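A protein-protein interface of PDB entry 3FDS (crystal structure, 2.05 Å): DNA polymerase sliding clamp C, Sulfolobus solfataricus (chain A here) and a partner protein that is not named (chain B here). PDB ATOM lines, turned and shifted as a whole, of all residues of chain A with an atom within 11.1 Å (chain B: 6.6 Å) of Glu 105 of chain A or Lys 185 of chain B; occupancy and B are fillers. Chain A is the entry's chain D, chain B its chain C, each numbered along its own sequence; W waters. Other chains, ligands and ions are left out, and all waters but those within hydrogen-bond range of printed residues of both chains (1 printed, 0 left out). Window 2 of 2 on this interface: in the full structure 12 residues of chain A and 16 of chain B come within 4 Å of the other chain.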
ATOM      1  N   ARG A  82     -13.356   2.381   6.850  1.00  0.00           N
ATOM      2  CA  ARG A  82     -13.504   3.554   7.727  1.00  0.00           C
ATOM      3  C   ARG A  82     -12.646   4.741   7.264  1.00  0.00           C
ATOM      4  O   ARG A  82     -12.712   5.838   7.851  1.00  0.00           O
ATOM      5  CB  ARG A  82     -13.209   3.204   9.179  1.00  0.00           C
ATOM      6  CG  ARG A  82     -14.226   2.147   9.797  1.00  0.00           C
ATOM      7  CD  ARG A  82     -15.750   2.631   9.864  1.00  0.00           C
ATOM      8  NE  ARG A  82     -15.832   4.000  10.308  1.00  0.00           N
ATOM      9  CZ  ARG A  82     -16.443   4.996   9.663  1.00  0.00           C
ATOM     10  NH1 ARG A  82     -16.392   6.248  10.171  1.00  0.00           N
ATOM     11  NH2 ARG A  82     -17.155   4.745   8.549  1.00  0.00           N
ATOM     12  N   VAL A  83     -11.847   4.510   6.201  1.00  0.00           N
ATOM     13  CA  VAL A  83     -10.990   5.584   5.637  1.00  0.00           C
ATOM     14  C   VAL A  83     -11.843   6.782   5.167  1.00  0.00           C
ATOM     15  O   VAL A  83     -12.904   6.596   4.566  1.00  0.00           O
ATOM     16  CB  VAL A  83     -10.055   5.042   4.505  1.00  0.00           C
ATOM     17  CG1 VAL A  83     -10.852   4.639   3.261  1.00  0.00           C
ATOM     18  CG2 VAL A  83      -8.959   6.077   4.120  1.00  0.00           C
ATOM     19  N   LEU A  84     -11.391   8.010   5.472  1.00  0.00           N
ATOM     20  CA  LEU A  84     -12.045   9.232   5.045  1.00  0.00           C
ATOM     21  C   LEU A  84     -11.351   9.857   3.798  1.00  0.00           C
ATOM     22  O   LEU A  84     -10.194   9.521   3.483  1.00  0.00           O
ATOM     23  CB  LEU A  84     -12.009  10.255   6.174  1.00  0.00           C
ATOM     24  CG  LEU A  84     -13.056  10.301   7.301  1.00  0.00           C
ATOM     25  CD1 LEU A  84     -14.053   9.102   7.380  1.00  0.00           C
ATOM     26  CD2 LEU A  84     -12.396  10.616   8.602  1.00  0.00           C
ATOM     27  N   LYS A  85     -12.040  10.785   3.140  1.00  0.00           N
ATOM     28  CA  LYS A  85     -11.514  11.421   1.901  1.00  0.00           C
ATOM     29  C   LYS A  85     -10.042  11.871   1.990  1.00  0.00           C
ATOM     30  O   LYS A  85      -9.228  11.464   1.154  1.00  0.00           O
ATOM     31  CB  LYS A  85     -12.409  12.549   1.376  1.00  0.00           C
ATOM     32  CG  LYS A  85     -11.854  13.267   0.081  1.00  0.00           C
ATOM     33  CD  LYS A  85     -12.927  13.943  -0.686  1.00  0.00           C
ATOM     34  CE  LYS A  85     -12.405  14.811  -1.889  1.00  0.00           C
ATOM     35  NZ  LYS A  85     -11.506  15.867  -1.289  1.00  0.00           N
ATOM     36  N   ASP A  86      -9.698  12.674   2.984  1.00  0.00           N
ATOM     37  CA  ASP A  86      -8.327  13.188   3.032  1.00  0.00           C
ATOM     38  C   ASP A  86      -7.338  12.405   3.933  1.00  0.00           C
ATOM     39  O   ASP A  86      -6.300  12.959   4.333  1.00  0.00           O
ATOM     40  CB  ASP A  86      -8.348  14.705   3.345  1.00  0.00           C
ATOM     41  CG  ASP A  86      -9.044  15.506   2.251  1.00  0.00           C
ATOM     42  OD1 ASP A  86      -9.820  16.451   2.580  1.00  0.00           O
ATOM     43  OD2 ASP A  86      -8.782  15.192   1.055  1.00  0.00           O
ATOM     44  N   ASP A  87      -7.615  11.113   4.196  1.00  0.00           N
ATOM     45  CA  ASP A  87      -6.821  10.392   5.184  1.00  0.00           C
ATOM     46  C   ASP A  87      -5.550   9.851   4.571  1.00  0.00           C
ATOM     47  O   ASP A  87      -5.554   9.371   3.426  1.00  0.00           O
ATOM     48  CB  ASP A  87      -7.558   9.176   5.757  1.00  0.00           C
ATOM     49  CG  ASP A  87      -8.550   9.522   6.891  1.00  0.00           C
ATOM     50  OD1 ASP A  87      -9.359   8.614   7.224  1.00  0.00           O
ATOM     51  OD2 ASP A  87      -8.520  10.638   7.459  1.00  0.00           O
ATOM     52  N   THR A  88      -4.478   9.867   5.344  1.00  0.00           N
ATOM     53  CA  THR A  88      -3.342   9.045   5.004  1.00  0.00           C
ATOM     54  C   THR A  88      -3.466   7.785   5.833  1.00  0.00           C
ATOM     55  O   THR A  88      -3.793   7.862   6.999  1.00  0.00           O
ATOM     56  CB  THR A  88      -2.031   9.709   5.410  1.00  0.00           C
ATOM     57  OG1 THR A  88      -1.746  10.763   4.486  1.00  0.00           O
ATOM     58  CG2 THR A  88      -0.905   8.724   5.311  1.00  0.00           C
ATOM     59  N   LEU A  89      -3.215   6.646   5.226  1.00  0.00           N
ATOM     60  CA  LEU A  89      -3.193   5.388   5.965  1.00  0.00           C
ATOM     61  C   LEU A  89      -1.753   4.942   6.288  1.00  0.00           C
ATOM     62  O   LEU A  89      -0.894   4.867   5.402  1.00  0.00           O
ATOM     63  CB  LEU A  89      -3.851   4.317   5.140  1.00  0.00           C
ATOM     64  CG  LEU A  89      -3.701   2.832   5.514  1.00  0.00           C
ATOM     65  CD1 LEU A  89      -4.451   2.538   6.810  1.00  0.00           C
ATOM     66  CD2 LEU A  89      -4.294   2.026   4.272  1.00  0.00           C
ATOM     67  N   ILE A  90      -1.514   4.598   7.544  1.00  0.00           N
ATOM     68  CA  ILE A  90      -0.200   4.105   7.948  1.00  0.00           C
ATOM     69  C   ILE A  90      -0.401   2.760   8.645  1.00  0.00           C
ATOM     70  O   ILE A  90      -1.210   2.648   9.601  1.00  0.00           O
ATOM     71  CB  ILE A  90       0.518   5.071   8.923  1.00  0.00           C
ATOM     72  CG1 ILE A  90       0.688   6.468   8.334  1.00  0.00           C
ATOM     73  CG2 ILE A  90       1.927   4.539   9.291  1.00  0.00           C
ATOM     74  CD1 ILE A  90      -0.287   7.482   8.930  1.00  0.00           C
ATOM     75  N   THR A 101      -3.663   3.225  11.176  1.00  0.00           N
ATOM     76  CA  THR A 101      -3.871   4.624  11.562  1.00  0.00           C
ATOM     77  C   THR A 101      -4.248   5.474  10.330  1.00  0.00           C
ATOM     78  O   THR A 101      -3.546   5.448   9.281  1.00  0.00           O
ATOM     79  CB  THR A 101      -2.595   5.213  12.188  1.00  0.00           C
ATOM     80  OG1 THR A 101      -2.190   4.343  13.258  1.00  0.00           O
ATOM     81  CG2 THR A 101      -2.802   6.663  12.738  1.00  0.00           C
ATOM     82  N   PHE A 102      -5.342   6.227  10.490  1.00  0.00           N
ATOM     83  CA  PHE A 102      -5.826   7.203   9.510  1.00  0.00           C
ATOM     84  C   PHE A 102      -5.496   8.595  10.039  1.00  0.00           C
ATOM     85  O   PHE A 102      -5.989   9.010  11.086  1.00  0.00           O
ATOM     86  CB  PHE A 102      -7.337   7.064   9.304  1.00  0.00           C
ATOM     87  CG  PHE A 102      -7.768   5.709   8.787  1.00  0.00           C
ATOM     88  CD1 PHE A 102      -8.626   4.913   9.535  1.00  0.00           C
ATOM     89  CD2 PHE A 102      -7.331   5.239   7.548  1.00  0.00           C
ATOM     90  CE1 PHE A 102      -9.011   3.658   9.091  1.00  0.00           C
ATOM     91  CE2 PHE A 102      -7.726   3.949   7.080  1.00  0.00           C
ATOM     92  CZ  PHE A 102      -8.576   3.168   7.880  1.00  0.00           C
ATOM     93  N   ASP A 103      -4.638   9.298   9.305  1.00  0.00           N
ATOM     94  CA  ASP A 103      -4.187  10.620   9.687  1.00  0.00           C
ATOM     95  C   ASP A 103      -4.783  11.587   8.656  1.00  0.00           C
ATOM     96  O   ASP A 103      -4.489  11.495   7.451  1.00  0.00           O
ATOM     97  CB  ASP A 103      -2.664  10.615   9.633  1.00  0.00           C
ATOM     98  CG  ASP A 103      -2.055  11.810  10.254  1.00  0.00           C
ATOM     99  OD1 ASP A 103      -0.835  12.013   9.969  1.00  0.00           O
ATOM    100  OD2 ASP A 103      -2.755  12.540  11.003  1.00  0.00           O
ATOM    101  N   GLY A 104      -5.631  12.488   9.121  1.00  0.00           N
ATOM    102  CA  GLY A 104      -6.436  13.299   8.211  1.00  0.00           C
ATOM    103  C   GLY A 104      -6.842  14.544   8.941  1.00  0.00           C
ATOM    104  O   GLY A 104      -6.022  15.201   9.548  1.00  0.00           O
ATOM    105  N   GLU A 105      -8.130  14.854   8.926  1.00  0.00           N
ATOM    106  CA  GLU A 105      -8.613  16.029   9.658  1.00  0.00           C
ATOM    107  C   GLU A 105      -8.445  15.848  11.176  1.00  0.00           C
ATOM    108  O   GLU A 105      -8.320  16.806  11.914  1.00  0.00           O
ATOM    109  CB  GLU A 105     -10.039  16.366   9.203  1.00  0.00           C
ATOM    110  CG  GLU A 105     -10.010  17.090   7.831  1.00  0.00           C
ATOM    111  CD  GLU A 105     -11.342  17.116   7.053  1.00  0.00           C
ATOM    112  OE1 GLU A 105     -11.886  18.234   6.871  1.00  0.00           O
ATOM    113  OE2 GLU A 105     -11.816  16.054   6.582  1.00  0.00           O
ATOM    114  N   PHE A 106      -8.391  14.599  11.628  1.00  0.00           N
ATOM    115  CA  PHE A 106      -7.823  14.262  12.948  1.00  0.00           C
ATOM    116  C   PHE A 106      -7.310  12.816  12.899  1.00  0.00           C
ATOM    117  O   PHE A 106      -7.451  12.173  11.885  1.00  0.00           O
ATOM    118  CB  PHE A 106      -8.845  14.448  14.074  1.00  0.00           C
ATOM    119  CG  PHE A 106     -10.111  13.647  13.912  1.00  0.00           C
ATOM    120  CD1 PHE A 106     -11.116  14.082  13.053  1.00  0.00           C
ATOM    121  CD2 PHE A 106     -10.322  12.470  14.652  1.00  0.00           C
ATOM    122  CE1 PHE A 106     -12.303  13.360  12.906  1.00  0.00           C
ATOM    123  CE2 PHE A 106     -11.517  11.768  14.546  1.00  0.00           C
ATOM    124  CZ  PHE A 106     -12.507  12.205  13.643  1.00  0.00           C
ATOM    125  N   THR A 107      -6.726  12.323  13.988  1.00  0.00           N
ATOM    126  CA  THR A 107      -6.047  11.037  13.970  1.00  0.00           C
ATOM    127  C   THR A 107      -6.876   9.957  14.648  1.00  0.00           C
ATOM    128  O   THR A 107      -7.376  10.200  15.720  1.00  0.00           O
ATOM    129  CB  THR A 107      -4.626  11.132  14.677  1.00  0.00           C
ATOM    130  OG1 THR A 107      -3.834  12.090  13.975  1.00  0.00           O
ATOM    131  CG2 THR A 107      -3.887   9.790  14.610  1.00  0.00           C
ATOM    132  N   ARG A 108      -6.947   8.771  14.028  1.00  0.00           N
ATOM    133  CA  ARG A 108      -7.769   7.642  14.464  1.00  0.00           C
ATOM    134  C   ARG A 108      -6.955   6.379  14.195  1.00  0.00           C
ATOM    135  O   ARG A 108      -6.566   6.180  13.058  1.00  0.00           O
ATOM    136  CB  ARG A 108      -9.106   7.563  13.599  1.00  0.00           C
ATOM    137  CG  ARG A 108     -10.068   8.774  13.702  1.00  0.00           C
ATOM    138  CD  ARG A 108     -11.256   8.794  12.663  1.00  0.00           C
ATOM    139  NE  ARG A 108     -10.816   8.581  11.278  1.00  0.00           N
ATOM    140  CZ  ARG A 108     -11.285   7.686  10.415  1.00  0.00           C
ATOM    141  NH1 ARG A 108     -12.291   6.858  10.708  1.00  0.00           N
ATOM    142  NH2 ARG A 108     -10.741   7.627   9.222  1.00  0.00           N
ATOM    143  N   PHE B 180      -7.936  11.027  18.725  1.00  0.00           N
ATOM    144  CA  PHE B 180      -7.591  12.280  19.420  1.00  0.00           C
ATOM    145  C   PHE B 180      -8.205  13.477  18.707  1.00  0.00           C
ATOM    146  O   PHE B 180      -8.047  13.647  17.483  1.00  0.00           O
ATOM    147  CB  PHE B 180      -6.072  12.431  19.561  1.00  0.00           C
ATOM    148  CG  PHE B 180      -5.462  11.438  20.506  1.00  0.00           C
ATOM    149  CD1 PHE B 180      -5.449  11.674  21.879  1.00  0.00           C
ATOM    150  CD2 PHE B 180      -4.913  10.248  20.028  1.00  0.00           C
ATOM    151  CE1 PHE B 180      -4.905  10.746  22.750  1.00  0.00           C
ATOM    152  CE2 PHE B 180      -4.356   9.309  20.900  1.00  0.00           C
ATOM    153  CZ  PHE B 180      -4.351   9.559  22.258  1.00  0.00           C
ATOM    154  N   LEU B 181      -8.935  14.282  19.468  1.00  0.00           N
ATOM    155  CA  LEU B 181      -9.493  15.518  18.968  1.00  0.00           C
ATOM    156  C   LEU B 181      -8.841  16.717  19.676  1.00  0.00           C
ATOM    157  O   LEU B 181      -8.730  16.737  20.898  1.00  0.00           O
ATOM    158  CB  LEU B 181     -11.008  15.560  19.184  1.00  0.00           C
ATOM    159  CG  LEU B 181     -11.880  14.372  18.810  1.00  0.00           C
ATOM    160  CD1 LEU B 181     -13.360  14.622  19.166  1.00  0.00           C
ATOM    161  CD2 LEU B 181     -11.758  14.087  17.322  1.00  0.00           C
ATOM    162  N   MET B 182      -8.441  17.727  18.921  1.00  0.00           N
ATOM    163  CA  MET B 182      -7.908  18.951  19.559  1.00  0.00           C
ATOM    164  C   MET B 182      -8.410  20.190  18.854  1.00  0.00           C
ATOM    165  O   MET B 182      -9.075  20.079  17.812  1.00  0.00           O
ATOM    166  CB  MET B 182      -6.365  18.951  19.665  1.00  0.00           C
ATOM    167  CG  MET B 182      -5.639  18.181  18.575  1.00  0.00           C
ATOM    168  SD  MET B 182      -3.865  17.970  18.907  1.00  0.00           S
ATOM    169  CE  MET B 182      -3.221  19.587  18.471  1.00  0.00           C
ATOM    170  N   LYS B 183      -8.105  21.351  19.430  1.00  0.00           N
ATOM    171  CA  LYS B 183      -8.505  22.624  18.866  1.00  0.00           C
ATOM    172  C   LYS B 183      -7.938  22.700  17.460  1.00  0.00           C
ATOM    173  O   LYS B 183      -6.749  22.483  17.249  1.00  0.00           O
ATOM    174  CB  LYS B 183      -8.006  23.780  19.738  1.00  0.00           C
ATOM    175  CG  LYS B 183      -8.931  25.028  19.710  1.00  0.00           C
ATOM    176  CD  LYS B 183      -8.880  25.801  21.044  1.00  0.00           C
ATOM    177  CE  LYS B 183      -9.664  27.136  20.946  1.00  0.00           C
ATOM    178  NZ  LYS B 183     -11.136  26.931  21.144  1.00  0.00           N
ATOM    179  N   ASP B 184      -8.826  22.949  16.506  1.00  0.00           N
ATOM    180  CA  ASP B 184      -8.494  23.119  15.089  1.00  0.00           C
ATOM    181  C   ASP B 184      -8.142  21.824  14.348  1.00  0.00           C
ATOM    182  O   ASP B 184      -7.837  21.868  13.156  1.00  0.00           O
ATOM    183  CB  ASP B 184      -7.402  24.175  14.882  1.00  0.00           C
ATOM    184  CG  ASP B 184      -7.797  25.556  15.406  1.00  0.00           C
ATOM    185  OD1 ASP B 184      -6.867  26.327  15.715  1.00  0.00           O
ATOM    186  OD2 ASP B 184      -9.010  25.891  15.491  1.00  0.00           O
ATOM    187  N   LYS B 185      -8.158  20.693  15.051  1.00  0.00           N
ATOM    188  CA  LYS B 185      -7.957  19.360  14.467  1.00  0.00           C
ATOM    189  C   LYS B 185      -8.772  18.344  15.267  1.00  0.00           C
ATOM    190  O   LYS B 185      -8.210  17.575  16.028  1.00  0.00           O
ATOM    191  CB  LYS B 185      -6.468  18.944  14.536  1.00  0.00           C
ATOM    192  CG  LYS B 185      -5.501  19.881  13.908  1.00  0.00           C
ATOM    193  CD  LYS B 185      -4.129  19.856  14.647  1.00  0.00           C
ATOM    194  CE  LYS B 185      -3.743  21.256  15.157  1.00  0.00           C
ATOM    195  NZ  LYS B 185      -2.331  21.303  15.683  1.00  0.00           N
ATOM    196  N   PRO B 186     -10.113  18.328  15.117  1.00  0.00           N
ATOM    197  CA  PRO B 186     -10.878  19.144  14.212  1.00  0.00           C
ATOM    198  C   PRO B 186     -11.701  20.192  14.976  1.00  0.00           C
ATOM    199  O   PRO B 186     -12.486  20.881  14.368  1.00  0.00           O
ATOM    200  CB  PRO B 186     -11.824  18.120  13.596  1.00  0.00           C
ATOM    201  CG  PRO B 186     -12.216  17.273  14.851  1.00  0.00           C
ATOM    202  CD  PRO B 186     -10.975  17.323  15.772  1.00  0.00           C
ATOM    203  N   LEU B 187     -11.529  20.278  16.294  1.00  0.00           N
ATOM    204  CA  LEU B 187     -12.478  20.998  17.154  1.00  0.00           C
ATOM    205  C   LEU B 187     -12.522  22.496  16.883  1.00  0.00           C
ATOM    206  O   LEU B 187     -11.487  23.138  16.686  1.00  0.00           O
ATOM    207  CB  LEU B 187     -12.178  20.746  18.634  1.00  0.00           C
ATOM    208  CG  LEU B 187     -12.171  19.274  19.096  1.00  0.00           C
ATOM    209  CD1 LEU B 187     -11.653  19.116  20.549  1.00  0.00           C
ATOM    210  CD2 LEU B 187     -13.550  18.640  18.900  1.00  0.00           C
ATOM    211  N   LYS B 188     -13.739  23.026  16.885  1.00  0.00           N
ATOM    212  CA  LYS B 188     -13.987  24.442  16.739  1.00  0.00           C
ATOM    213  C   LYS B 188     -13.641  25.133  18.053  1.00  0.00           C
ATOM    214  O   LYS B 188     -13.093  26.211  18.050  1.00  0.00           O
ATOM    215  CB  LYS B 188     -15.457  24.699  16.382  1.00  0.00           C
ATOM    216  CG  LYS B 188     -15.871  24.247  15.008  1.00  0.00           C
ATOM    217  CD  LYS B 188     -17.418  24.304  14.913  1.00  0.00           C
ATOM    218  CE  LYS B 188     -17.946  23.737  13.597  1.00  0.00           C
ATOM    219  NZ  LYS B 188     -17.622  24.636  12.429  1.00  0.00           N
HETATM  220  O   HOH W   1      -6.076  14.573  16.070  1.00  0.00           O
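The side-chain carboxylate of Asp 103 of chain A lies within hydrogen-bond range of the side-chain hydroxyl of Thr 107 of chain A, 3.2 Å away.
Of the 17 printed residues of chain A, 3 touch a printed residue of chain B. Hydrophobic or aromatic side chains of chain A that line the printed part of chain B: Phe 106. Of the 9 printed residues of chain B, 4 touch a printed residue of chain A. Hydrophobic or aromatic side chains of chain B that line the printed part of chain A: Leu 181 and Pro 186. Among the printed residues, 7 pairs touch across the chains. Among the printed residues, no Asp or Glu carboxylate lies within 4 Å of a Lys or Arg side-chain nitrogen of the other chain.
Water W1 bridges O of Phe 180 of chain B and N of Thr 107 of chain A.
Among the printed residues, pairs that only touch across the chains: Phe 106 of chain A with Leu 181 of chain B (3.4 Å), Phe 106 of chain A with Phe 180 of chain B (3.6 Å), Glu 105 of chain A with Lys 185 of chain B (3.6 Å), Phe 106 of chain A with Lys 185 of chain B (3.7 Å), Phe 106 of chain A with Pro 186 of chain B (3.8 Å) and Glu 105 of chain A with Pro 186 of chain B (3.97 Å).
N of Phe 180 of chain B lies within hydrogen-bond range of O of Thr 107 of chain A (3.2 Å).
Glu 105 of chain A touches just these residues of chain B: Lys 185 and Pro 186. Lys 185 of chain B touches two residues of chain A. Of chain A, only Phe 106 (3.4 Å) comes within 4 Å of Leu 181 of chain B. No residue of chain A comes within 4 Å of Met 182 of chain B. No residue of chain A comes within 4 Å of Asp 184 of chain B. Of chain A, only Glu 105 (3.97 Å) and Phe 106 (3.8 Å) come within 4 Å of Pro 186 of chain B. No residue of chain A comes within 4 Å of Leu 187 of chain B. Of the printed residues of chain A, Phe 180 of chain B touches Phe 106 and Thr 107. Of the printed residues of chain B, Phe 106 of chain A touches Phe 180 (3.6 Å), Leu 181 (3.4 Å), Lys 185 (3.7 Å) and Pro 186 (3.8 Å). Printed residues of chain B within 4 Å of Thr 107 of chain A: Phe 180.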
